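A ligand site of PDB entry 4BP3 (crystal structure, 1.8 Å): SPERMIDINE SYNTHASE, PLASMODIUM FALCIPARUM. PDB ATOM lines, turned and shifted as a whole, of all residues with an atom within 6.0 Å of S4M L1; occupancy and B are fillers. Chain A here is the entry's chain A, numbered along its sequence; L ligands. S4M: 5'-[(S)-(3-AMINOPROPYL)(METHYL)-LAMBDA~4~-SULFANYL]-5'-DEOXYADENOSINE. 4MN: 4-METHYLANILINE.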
ATOM      1  N   GLN A  34     -22.134  19.918  -6.794  1.00  0.00           N
ATOM      2  CA  GLN A  34     -21.060  20.752  -7.187  1.00  0.00           C
ATOM      3  C   GLN A  34     -20.791  21.955  -6.301  1.00  0.00           C
ATOM      4  O   GLN A  34     -21.580  22.310  -5.451  1.00  0.00           O
ATOM      5  CB  GLN A  34     -21.281  21.079  -8.684  1.00  0.00           C
ATOM      6  CG  GLN A  34     -22.359  21.979  -9.019  1.00  0.00           C
ATOM      7  CD  GLN A  34     -23.059  21.690 -10.415  1.00  0.00           C
ATOM      8  OE1 GLN A  34     -22.487  21.540 -11.526  1.00  0.00           O
ATOM      9  NE2 GLN A  34     -24.372  21.692 -10.319  1.00  0.00           N
ATOM     10  N   LEU A  48     -22.345  33.345 -11.878  1.00  0.00           N
ATOM     11  CA  LEU A  48     -22.553  32.048 -11.255  1.00  0.00           C
ATOM     12  C   LEU A  48     -21.469  31.146 -11.761  1.00  0.00           C
ATOM     13  O   LEU A  48     -21.213  31.070 -12.980  1.00  0.00           O
ATOM     14  CB  LEU A  48     -23.948  31.511 -11.693  1.00  0.00           C
ATOM     15  CG  LEU A  48     -24.191  30.053 -11.365  1.00  0.00           C
ATOM     16  CD1 LEU A  48     -24.283  29.982  -9.841  1.00  0.00           C
ATOM     17  CD2 LEU A  48     -25.469  29.491 -11.950  1.00  0.00           C
ATOM     18  N   LEU A  50     -19.763  27.159 -11.194  1.00  0.00           N
ATOM     19  CA  LEU A  50     -19.947  25.775 -10.739  1.00  0.00           C
ATOM     20  C   LEU A  50     -18.684  24.926 -10.994  1.00  0.00           C
ATOM     21  O   LEU A  50     -18.153  24.858 -12.130  1.00  0.00           O
ATOM     22  CB  LEU A  50     -21.130  25.166 -11.445  1.00  0.00           C
ATOM     23  CG  LEU A  50     -22.515  25.785 -11.268  1.00  0.00           C
ATOM     24  CD1 LEU A  50     -23.561  25.049 -12.118  1.00  0.00           C
ATOM     25  CD2 LEU A  50     -22.970  25.721  -9.817  1.00  0.00           C
ATOM     26  N   GLN A  55     -20.483  29.687 -15.388  1.00  0.00           N
ATOM     27  CA  GLN A  55     -21.758  29.269 -16.053  1.00  0.00           C
ATOM     28  C   GLN A  55     -22.526  30.384 -16.686  1.00  0.00           C
ATOM     29  O   GLN A  55     -23.177  30.208 -17.735  1.00  0.00           O
ATOM     30  CB  GLN A  55     -22.691  28.581 -15.041  1.00  0.00           C
ATOM     31  CG  GLN A  55     -22.012  27.458 -14.338  1.00  0.00           C
ATOM     32  CD  GLN A  55     -21.664  26.293 -15.236  1.00  0.00           C
ATOM     33  OE1 GLN A  55     -22.520  25.797 -15.945  1.00  0.00           O
ATOM     34  NE2 GLN A  55     -20.412  25.873 -15.226  1.00  0.00           N
ATOM     35  N   LEU A  56     -22.515  31.519 -16.058  1.00  0.00           N
ATOM     36  CA  LEU A  56     -23.115  32.682 -16.623  1.00  0.00           C
ATOM     37  C   LEU A  56     -22.734  33.940 -15.921  1.00  0.00           C
ATOM     38  O   LEU A  56     -22.255  33.930 -14.798  1.00  0.00           O
ATOM     39  CB  LEU A  56     -24.644  32.562 -16.703  1.00  0.00           C
ATOM     40  CG  LEU A  56     -25.450  32.597 -15.409  1.00  0.00           C
ATOM     41  CD1 LEU A  56     -25.618  33.967 -14.854  1.00  0.00           C
ATOM     42  CD2 LEU A  56     -26.868  32.063 -15.688  1.00  0.00           C
ATOM     43  N   TYR A  64     -25.911  33.432 -25.138  1.00  0.00           N
ATOM     44  CA  TYR A  64     -26.024  32.017 -25.148  1.00  0.00           C
ATOM     45  C   TYR A  64     -27.538  31.625 -24.986  1.00  0.00           C
ATOM     46  O   TYR A  64     -27.992  30.751 -25.681  1.00  0.00           O
ATOM     47  CB  TYR A  64     -25.273  31.447 -23.976  1.00  0.00           C
ATOM     48  CG  TYR A  64     -25.441  30.025 -23.735  1.00  0.00           C
ATOM     49  CD1 TYR A  64     -24.735  29.086 -24.446  1.00  0.00           C
ATOM     50  CD2 TYR A  64     -26.289  29.571 -22.715  1.00  0.00           C
ATOM     51  CE1 TYR A  64     -24.836  27.754 -24.168  1.00  0.00           C
ATOM     52  CE2 TYR A  64     -26.416  28.209 -22.455  1.00  0.00           C
ATOM     53  CZ  TYR A  64     -25.715  27.319 -23.153  1.00  0.00           C
ATOM     54  OH  TYR A  64     -25.794  25.954 -22.912  1.00  0.00           O
ATOM     55  N   HIS A  65     -28.276  32.325 -24.113  1.00  0.00           N
ATOM     56  CA  HIS A  65     -29.707  31.953 -23.875  1.00  0.00           C
ATOM     57  C   HIS A  65     -30.565  32.166 -25.092  1.00  0.00           C
ATOM     58  O   HIS A  65     -31.304  31.251 -25.502  1.00  0.00           O
ATOM     59  CB  HIS A  65     -30.258  32.628 -22.632  1.00  0.00           C
ATOM     60  CG  HIS A  65     -29.627  32.076 -21.407  1.00  0.00           C
ATOM     61  ND1 HIS A  65     -29.119  32.879 -20.410  1.00  0.00           N
ATOM     62  CD2 HIS A  65     -29.335  30.805 -21.066  1.00  0.00           C
ATOM     63  CE1 HIS A  65     -28.558  32.113 -19.501  1.00  0.00           C
ATOM     64  NE2 HIS A  65     -28.649  30.861 -19.891  1.00  0.00           N
ATOM     65  N   VAL A  85     -32.770  20.580 -20.511  1.00  0.00           N
ATOM     66  CA  VAL A  85     -31.836  19.839 -19.716  1.00  0.00           C
ATOM     67  C   VAL A  85     -30.803  20.762 -19.117  1.00  0.00           C
ATOM     68  O   VAL A  85     -30.284  21.624 -19.805  1.00  0.00           O
ATOM     69  CB  VAL A  85     -31.154  18.743 -20.537  1.00  0.00           C
ATOM     70  CG1 VAL A  85     -29.977  18.045 -19.844  1.00  0.00           C
ATOM     71  CG2 VAL A  85     -32.185  17.732 -20.966  1.00  0.00           C
ATOM     72  N   GLY A  86     -30.502  20.593 -17.823  1.00  0.00           N
ATOM     73  CA  GLY A  86     -29.678  21.548 -17.135  1.00  0.00           C
ATOM     74  C   GLY A  86     -30.422  22.832 -17.000  1.00  0.00           C
ATOM     75  O   GLY A  86     -31.583  22.857 -16.670  1.00  0.00           O
ATOM     76  N   GLY A  87     -29.775  23.940 -17.280  1.00  0.00           N
ATOM     77  CA  GLY A  87     -30.465  25.203 -17.323  1.00  0.00           C
ATOM     78  C   GLY A  87     -31.134  25.754 -16.045  1.00  0.00           C
ATOM     79  O   GLY A  87     -32.033  26.616 -16.102  1.00  0.00           O
ATOM     80  N   GLY A  88     -30.590  25.444 -14.881  1.00  0.00           N
ATOM     81  CA  GLY A  88     -31.283  25.795 -13.615  1.00  0.00           C
ATOM     82  C   GLY A  88     -31.361  27.239 -13.337  1.00  0.00           C
ATOM     83  O   GLY A  88     -32.262  27.736 -12.623  1.00  0.00           O
ATOM     84  N   ASP A  89     -30.458  27.991 -13.950  1.00  0.00           N
ATOM     85  CA  ASP A  89     -30.564  29.414 -13.832  1.00  0.00           C
ATOM     86  C   ASP A  89     -31.895  30.004 -14.348  1.00  0.00           C
ATOM     87  O   ASP A  89     -32.337  31.104 -13.924  1.00  0.00           O
ATOM     88  CB  ASP A  89     -29.338  30.016 -14.555  1.00  0.00           C
ATOM     89  CG  ASP A  89     -29.198  29.457 -15.952  1.00  0.00           C
ATOM     90  OD1 ASP A  89     -29.876  29.986 -16.763  1.00  0.00           O
ATOM     91  OD2 ASP A  89     -28.524  28.431 -16.196  1.00  0.00           O
ATOM     92  N   GLY A  91     -32.486  30.827 -17.610  1.00  0.00           N
ATOM     93  CA  GLY A  91     -32.337  31.728 -18.763  1.00  0.00           C
ATOM     94  C   GLY A  91     -33.058  31.222 -20.016  1.00  0.00           C
ATOM     95  O   GLY A  91     -33.746  31.968 -20.697  1.00  0.00           O
ATOM     96  N   ILE A  92     -32.931  29.945 -20.261  1.00  0.00           N
ATOM     97  CA  ILE A  92     -33.582  29.315 -21.375  1.00  0.00           C
ATOM     98  C   ILE A  92     -35.107  29.376 -21.191  1.00  0.00           C
ATOM     99  O   ILE A  92     -35.843  29.738 -22.099  1.00  0.00           O
ATOM    100  CB  ILE A  92     -33.145  27.843 -21.576  1.00  0.00           C
ATOM    101  CG1 ILE A  92     -31.614  27.644 -21.950  1.00  0.00           C
ATOM    102  CG2 ILE A  92     -33.904  27.248 -22.693  1.00  0.00           C
ATOM    103  CD1 ILE A  92     -31.221  28.438 -23.212  1.00  0.00           C
ATOM    104  N   CYS A 108     -35.387  19.809 -16.449  1.00  0.00           N
ATOM    105  CA  CYS A 108     -34.735  18.782 -15.697  1.00  0.00           C
ATOM    106  C   CYS A 108     -33.304  19.267 -15.341  1.00  0.00           C
ATOM    107  O   CYS A 108     -32.424  19.289 -16.206  1.00  0.00           O
ATOM    108  CB  CYS A 108     -34.624  17.545 -16.436  1.00  0.00           C
ATOM    109  SG  CYS A 108     -33.965  16.190 -15.435  1.00  0.00           S
ATOM    110  N   GLU A 109     -33.125  19.670 -14.074  1.00  0.00           N
ATOM    111  CA  GLU A 109     -31.886  20.229 -13.547  1.00  0.00           C
ATOM    112  C   GLU A 109     -31.540  19.370 -12.385  1.00  0.00           C
ATOM    113  O   GLU A 109     -32.414  19.150 -11.514  1.00  0.00           O
ATOM    114  CB  GLU A 109     -32.167  21.668 -13.088  1.00  0.00           C
ATOM    115  CG  GLU A 109     -31.168  22.215 -12.079  1.00  0.00           C
ATOM    116  CD  GLU A 109     -29.742  22.285 -12.612  1.00  0.00           C
ATOM    117  OE1 GLU A 109     -29.457  23.130 -13.529  1.00  0.00           O
ATOM    118  OE2 GLU A 109     -28.905  21.448 -12.144  1.00  0.00           O
ATOM    119  N   ILE A 110     -30.318  18.834 -12.387  1.00  0.00           N
ATOM    120  CA  ILE A 110     -29.873  17.900 -11.395  1.00  0.00           C
ATOM    121  C   ILE A 110     -29.706  18.599 -10.002  1.00  0.00           C
ATOM    122  O   ILE A 110     -29.870  17.982  -8.959  1.00  0.00           O
ATOM    123  CB  ILE A 110     -28.573  17.221 -11.837  1.00  0.00           C
ATOM    124  CG1 ILE A 110     -28.235  15.975 -11.013  1.00  0.00           C
ATOM    125  CG2 ILE A 110     -27.368  18.188 -11.807  1.00  0.00           C
ATOM    126  CD1 ILE A 110     -27.078  15.122 -11.581  1.00  0.00           C
ATOM    127  N   ASP A 111     -29.454  19.876  -9.993  1.00  0.00           N
ATOM    128  CA  ASP A 111     -29.009  20.564  -8.759  1.00  0.00           C
ATOM    129  C   ASP A 111     -29.970  21.620  -8.328  1.00  0.00           C
ATOM    130  O   ASP A 111     -29.907  22.732  -8.835  1.00  0.00           O
ATOM    131  CB  ASP A 111     -27.579  21.114  -9.014  1.00  0.00           C
ATOM    132  CG  ASP A 111     -26.866  21.490  -7.715  1.00  0.00           C
ATOM    133  OD1 ASP A 111     -27.635  21.689  -6.727  1.00  0.00           O
ATOM    134  OD2 ASP A 111     -25.617  21.596  -7.713  1.00  0.00           O
ATOM    135  N   VAL A 114     -28.967  25.230  -7.666  1.00  0.00           N
ATOM    136  CA  VAL A 114     -28.765  26.170  -8.772  1.00  0.00           C
ATOM    137  C   VAL A 114     -30.051  27.001  -8.980  1.00  0.00           C
ATOM    138  O   VAL A 114     -30.037  28.253  -9.066  1.00  0.00           O
ATOM    139  CB  VAL A 114     -28.308  25.437 -10.023  1.00  0.00           C
ATOM    140  CG1 VAL A 114     -28.269  26.414 -11.179  1.00  0.00           C
ATOM    141  CG2 VAL A 114     -26.901  24.830  -9.832  1.00  0.00           C
ATOM    142  N   GLU A 139     -33.436  16.212 -11.067  1.00  0.00           N
ATOM    143  CA  GLU A 139     -32.908  14.884 -11.382  1.00  0.00           C
ATOM    144  C   GLU A 139     -31.781  14.944 -12.459  1.00  0.00           C
ATOM    145  O   GLU A 139     -31.721  15.909 -13.210  1.00  0.00           O
ATOM    146  CB  GLU A 139     -34.100  14.176 -12.089  1.00  0.00           C
ATOM    147  CG  GLU A 139     -33.998  12.701 -12.130  1.00  0.00           C
ATOM    148  CD  GLU A 139     -35.256  12.028 -12.700  1.00  0.00           C
ATOM    149  OE1 GLU A 139     -36.265  12.679 -13.094  1.00  0.00           O
ATOM    150  OE2 GLU A 139     -35.189  10.814 -12.717  1.00  0.00           O
ATOM    151  N   ASP A 140     -30.961  13.907 -12.547  1.00  0.00           N
ATOM    152  CA  ASP A 140     -29.992  13.711 -13.618  1.00  0.00           C
ATOM    153  C   ASP A 140     -30.774  13.542 -14.941  1.00  0.00           C
ATOM    154  O   ASP A 140     -31.582  12.660 -15.092  1.00  0.00           O
ATOM    155  CB  ASP A 140     -29.095  12.513 -13.342  1.00  0.00           C
ATOM    156  CG  ASP A 140     -27.883  12.359 -14.360  1.00  0.00           C
ATOM    157  OD1 ASP A 140     -27.987  12.692 -15.550  1.00  0.00           O
ATOM    158  OD2 ASP A 140     -26.806  11.813 -14.002  1.00  0.00           O
ATOM    159  N   ALA A 141     -30.529  14.399 -15.916  1.00  0.00           N
ATOM    160  CA  ALA A 141     -31.278  14.303 -17.180  1.00  0.00           C
ATOM    161  C   ALA A 141     -31.067  12.960 -17.860  1.00  0.00           C
ATOM    162  O   ALA A 141     -31.923  12.557 -18.646  1.00  0.00           O
ATOM    163  CB  ALA A 141     -30.982  15.433 -18.116  1.00  0.00           C
ATOM    164  N   SER A 142     -29.943  12.313 -17.613  1.00  0.00           N
ATOM    165  CA  SER A 142     -29.673  11.052 -18.180  1.00  0.00           C
ATOM    166  C   SER A 142     -30.775  10.045 -17.726  1.00  0.00           C
ATOM    167  O   SER A 142     -31.152   9.093 -18.468  1.00  0.00           O
ATOM    168  CB  SER A 142     -28.336  10.526 -17.684  1.00  0.00           C
ATOM    169  OG  SER A 142     -28.084   9.322 -18.373  1.00  0.00           O
ATOM    170  N   ASP A 158     -28.709  22.546 -22.039  1.00  0.00           N
ATOM    171  CA  ASP A 158     -27.985  23.628 -21.447  1.00  0.00           C
ATOM    172  C   ASP A 158     -27.156  23.079 -20.257  1.00  0.00           C
ATOM    173  O   ASP A 158     -27.507  23.332 -19.079  1.00  0.00           O
ATOM    174  CB  ASP A 158     -28.924  24.700 -21.007  1.00  0.00           C
ATOM    175  CG  ASP A 158     -28.213  25.858 -20.386  1.00  0.00           C
ATOM    176  OD1 ASP A 158     -26.980  25.914 -20.480  1.00  0.00           O
ATOM    177  OD2 ASP A 158     -28.844  26.727 -19.816  1.00  0.00           O
ATOM    178  N   SER A 159     -26.135  22.303 -20.595  1.00  0.00           N
ATOM    179  CA  SER A 159     -25.335  21.634 -19.608  1.00  0.00           C
ATOM    180  C   SER A 159     -24.050  22.377 -19.334  1.00  0.00           C
ATOM    181  O   SER A 159     -23.528  23.120 -20.151  1.00  0.00           O
ATOM    182  CB  SER A 159     -24.898  20.272 -20.065  1.00  0.00           C
ATOM    183  OG  SER A 159     -23.985  20.264 -21.179  1.00  0.00           O
ATOM    184  N   SER A 160     -23.496  22.082 -18.177  1.00  0.00           N
ATOM    185  CA  SER A 160     -22.094  22.388 -17.902  1.00  0.00           C
ATOM    186  C   SER A 160     -21.134  21.436 -18.707  1.00  0.00           C
ATOM    187  O   SER A 160     -21.544  20.676 -19.614  1.00  0.00           O
ATOM    188  CB  SER A 160     -21.910  22.292 -16.414  1.00  0.00           C
ATOM    189  OG  SER A 160     -22.578  21.151 -15.939  1.00  0.00           O
ATOM    190  N   GLY A 164     -17.664  16.659 -14.176  1.00  0.00           N
ATOM    191  CA  GLY A 164     -18.724  16.954 -13.217  1.00  0.00           C
ATOM    192  C   GLY A 164     -19.996  16.171 -13.606  1.00  0.00           C
ATOM    193  O   GLY A 164     -19.907  15.231 -14.415  1.00  0.00           O
ATOM    194  N   PRO A 165     -21.145  16.585 -13.061  1.00  0.00           N
ATOM    195  CA  PRO A 165     -22.391  15.788 -13.310  1.00  0.00           C
ATOM    196  C   PRO A 165     -22.833  15.756 -14.755  1.00  0.00           C
ATOM    197  O   PRO A 165     -23.596  14.923 -15.140  1.00  0.00           O
ATOM    198  CB  PRO A 165     -23.448  16.497 -12.442  1.00  0.00           C
ATOM    199  CG  PRO A 165     -22.907  17.887 -12.174  1.00  0.00           C
ATOM    200  CD  PRO A 165     -21.402  17.780 -12.188  1.00  0.00           C
ATOM    201  N   ALA A 166     -22.354  16.680 -15.586  1.00  0.00           N
ATOM    202  CA  ALA A 166     -22.685  16.621 -16.983  1.00  0.00           C
ATOM    203  C   ALA A 166     -21.961  15.549 -17.749  1.00  0.00           C
ATOM    204  O   ALA A 166     -22.171  15.363 -18.943  1.00  0.00           O
ATOM    205  CB  ALA A 166     -22.536  18.004 -17.618  1.00  0.00           C
ATOM    206  N   GLU A 167     -21.142  14.779 -17.068  1.00  0.00           N
ATOM    207  CA  GLU A 167     -20.402  13.679 -17.711  1.00  0.00           C
ATOM    208  C   GLU A 167     -21.333  12.694 -18.448  1.00  0.00           C
ATOM    209  O   GLU A 167     -20.971  12.200 -19.514  1.00  0.00           O
ATOM    210  CB  GLU A 167     -19.582  12.953 -16.675  1.00  0.00           C
ATOM    211  CG  GLU A 167     -18.628  11.985 -17.309  1.00  0.00           C
ATOM    212  CD  GLU A 167     -17.700  11.305 -16.322  1.00  0.00           C
ATOM    213  OE1 GLU A 167     -17.929  11.460 -15.064  1.00  0.00           O
ATOM    214  OE2 GLU A 167     -16.757  10.639 -16.841  1.00  0.00           O
ATOM    215  N   THR A 168     -22.507  12.439 -17.881  1.00  0.00           N
ATOM    216  CA  THR A 168     -23.488  11.562 -18.421  1.00  0.00           C
ATOM    217  C   THR A 168     -24.167  12.138 -19.639  1.00  0.00           C
ATOM    218  O   THR A 168     -24.981  11.446 -20.261  1.00  0.00           O
ATOM    219  CB  THR A 168     -24.591  11.292 -17.362  1.00  0.00           C
ATOM    220  OG1 THR A 168     -25.188  12.550 -17.047  1.00  0.00           O
ATOM    221  CG2 THR A 168     -24.031  10.620 -16.133  1.00  0.00           C
ATOM    222  N   LEU A 169     -23.931  13.397 -19.979  1.00  0.00           N
ATOM    223  CA  LEU A 169     -24.631  14.034 -21.078  1.00  0.00           C
ATOM    224  C   LEU A 169     -23.780  14.024 -22.415  1.00  0.00           C
ATOM    225  O   LEU A 169     -24.264  14.457 -23.409  1.00  0.00           O
ATOM    226  CB  LEU A 169     -25.079  15.425 -20.711  1.00  0.00           C
ATOM    227  CG  LEU A 169     -25.827  15.642 -19.368  1.00  0.00           C
ATOM    228  CD1 LEU A 169     -26.212  17.097 -19.128  1.00  0.00           C
ATOM    229  CD2 LEU A 169     -27.091  14.812 -19.340  1.00  0.00           C
ATOM    230  N   TYR A 226     -17.222  32.295 -21.757  1.00  0.00           N
ATOM    231  CA  TYR A 226     -16.856  30.951 -21.881  1.00  0.00           C
ATOM    232  C   TYR A 226     -15.445  30.837 -22.540  1.00  0.00           C
ATOM    233  O   TYR A 226     -15.007  31.728 -23.283  1.00  0.00           O
ATOM    234  CB  TYR A 226     -17.867  30.124 -22.679  1.00  0.00           C
ATOM    235  CG  TYR A 226     -19.244  30.042 -22.046  1.00  0.00           C
ATOM    236  CD1 TYR A 226     -19.387  29.742 -20.683  1.00  0.00           C
ATOM    237  CD2 TYR A 226     -20.353  30.093 -22.805  1.00  0.00           C
ATOM    238  CE1 TYR A 226     -20.633  29.580 -20.109  1.00  0.00           C
ATOM    239  CE2 TYR A 226     -21.616  29.994 -22.234  1.00  0.00           C
ATOM    240  CZ  TYR A 226     -21.769  29.743 -20.867  1.00  0.00           C
ATOM    241  OH  TYR A 226     -23.042  29.678 -20.268  1.00  0.00           O
HETATM  242  CA  S4M L   1     -26.076  28.967 -18.592  1.00  0.00           C
HETATM  243  N   S4M L   1     -27.481  28.621 -18.529  1.00  0.00           N
HETATM  244  CB  S4M L   1     -25.355  28.106 -17.569  1.00  0.00           C
HETATM  245  CG  S4M L   1     -25.702  26.624 -17.698  1.00  0.00           C
HETATM  246  SD  S4M L   1     -26.576  25.838 -16.456  1.00  0.00           S
HETATM  247  CE  S4M L   1     -26.578  26.798 -15.011  1.00  0.00           C
HETATM  248  C5' S4M L   1     -25.779  24.280 -16.459  1.00  0.00           C
HETATM  249  C4' S4M L   1     -26.586  23.272 -15.623  1.00  0.00           C
HETATM  250  O4' S4M L   1     -26.465  21.932 -16.053  1.00  0.00           O
HETATM  251  C1' S4M L   1     -26.752  21.133 -14.862  1.00  0.00           C
HETATM  252  C2' S4M L   1     -25.884  21.845 -13.834  1.00  0.00           C
HETATM  253  O2' S4M L   1     -26.203  21.581 -12.488  1.00  0.00           O
HETATM  254  C3' S4M L   1     -26.143  23.268 -14.142  1.00  0.00           C
HETATM  255  O3' S4M L   1     -27.088  23.972 -13.312  1.00  0.00           O
HETATM  256  N9  S4M L   1     -26.369  19.763 -15.067  1.00  0.00           N
HETATM  257  C8  S4M L   1     -25.133  19.222 -15.138  1.00  0.00           C
HETATM  258  N7  S4M L   1     -25.231  17.918 -15.354  1.00  0.00           N
HETATM  259  C5  S4M L   1     -26.575  17.649 -15.393  1.00  0.00           C
HETATM  260  C6  S4M L   1     -27.308  16.496 -15.558  1.00  0.00           C
HETATM  261  N6  S4M L   1     -26.615  15.343 -15.713  1.00  0.00           N
HETATM  262  C4  S4M L   1     -27.273  18.773 -15.198  1.00  0.00           C
HETATM  263  N3  S4M L   1     -28.644  18.821 -15.221  1.00  0.00           N
HETATM  264  C2  S4M L   1     -29.335  17.721 -15.379  1.00  0.00           C
HETATM  265  N1  S4M L   1     -28.670  16.559 -15.540  1.00  0.00           N
HETATM  266  N1  4MN L   2     -17.473  25.928 -20.008  1.00  0.00           N
HETATM  267  C5  4MN L   2     -18.826  26.029 -20.189  1.00  0.00           C
HETATM  268  C6  4MN L   2     -19.695  25.991 -19.078  1.00  0.00           C
HETATM  269  C4  4MN L   2     -19.346  26.187 -21.470  1.00  0.00           C
HETATM  270  C3  4MN L   2     -20.739  26.341 -21.651  1.00  0.00           C
HETATM  271  C2  4MN L   2     -21.612  26.282 -20.537  1.00  0.00           C
HETATM  272  C1  4MN L   2     -23.105  26.441 -20.664  1.00  0.00           C
HETATM  273  C7  4MN L   2     -21.086  26.117 -19.235  1.00  0.00           C
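The side-chain carboxylate (OD2) of Asp 89 is in salt-bridge range of a nitrogen (N) of S4M L1.
The backbone carbonyl oxygen (O) of Asp 158 sits close to a sulfur (SD) of S4M L1 (3.7 Å).
N of Ile 110 lies within hydrogen-bond range of N3 of S4M L1 (3.3 Å).
The backbone NH of Ala 141 is in hydrogen-bond range of a nitrogen (N1) of S4M L1 (2.9 Å).
A nitrogen (N) of S4M L1 lies within hydrogen-bond range of a ring nitrogen (NE2) of His 65 (2.9 Å).
The side-chain hydroxyl of Thr 168 lies within hydrogen-bond range of a nitrogen (N6) of S4M L1 (3.4 Å).
OE1 of Glu 109 lies within hydrogen-bond range of O3' of S4M L1, at 2.5 Å.
OD2 of Asp 158 is in salt-bridge range of N of S4M L1, at 2.7 Å.
The backbone NH (N) of Ala 166 lies within hydrogen-bond range of a nitrogen (N7) of S4M L1 (3.1 Å).
A nitrogen (N6) of S4M L1 is in hydrogen-bond range of the side-chain carboxylate (OD1) of Asp 140, at 3.0 Å.
The side-chain amide nitrogen (NE2) of Gln 34 is in hydrogen-bond range of an oxygen (O2') of S4M L1.
O of Pro 165 sits at hydrogen-bond distance from N6 of S4M L1.
The side-chain carboxylate of Glu 109 sits at hydrogen-bond distance from the backbone NH of Asp 111, 2.7 Å away.
The backbone carbonyl oxygen (O) of Pro 165 is in hydrogen-bond range of the side-chain hydroxyl (OG1) of Thr 168 (3.4 Å).
N of Gly 86 is in hydrogen-bond range of O of Cys 108 (2.8 Å).
The backbone NH of Gly 87 is in hydrogen-bond range of the backbone carbonyl oxygen of Asp 158 (3.0 Å).
The side-chain carboxylate (OD1) of Asp 140 lies within hydrogen-bond range of the backbone NH (N) of Ser 142 (2.9 Å).
N of Gly 91 lies within hydrogen-bond range of OD1 of Asp 89 (2.9 Å).
OD1 of Asp 89 lies within hydrogen-bond range of NE2 of His 65, at 3.5 Å.
N of Gln 55 lies within hydrogen-bond range of O of Leu 48 (2.9 Å).
Leu 50 touches S4M L1.
Gln 55 touches S4M L1 (O to CB, 3.0 Å).
Tyr 64 touches S4M L1 (CE2 to CA, 3.95 Å).
CA of Gly 86 touches O4' of S4M L1, at 3.4 Å.
N of Gly 87 touches C4' of S4M L1 (3.7 Å).
O of Cys 108 touches C2 of S4M L1, at 3.6 Å.
Asp 111 touches S4M L1.
Val 114 touches S4M L1 (CG1 to O3', 3.5 Å).
O of Glu 139 touches C2 of S4M L1, at 3.7 Å.
Ser 159 touches S4M L1 (CA to O4', 3.7 Å).
OG of Ser 160 touches C8 of S4M L1, 3.3 Å away.
CD2 of Leu 169 touches N6 of S4M L1, at 3.7 Å.
Tyr 226 touches S4M L1.
Hydrophobic or aromatic side chains within 4 Å of S4M L1: Leu 50, Tyr 64, His 65, Ile 110, Val 114, Ala 141, Pro 165, Ala 166 and Leu 169.
Within 4 Å of S4M L1: Gln 34, Leu 50, Gln 55, Tyr 64, His 65, Gly 86, Gly 87, Asp 89, Cys 108, Glu 109, Ile 110, Asp 111, Val 114, Glu 139, Asp 140, Ala 141, Asp 158, Ser 159, Ser 160, Pro 165, Ala 166, Thr 168, Leu 169 and Tyr 226.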
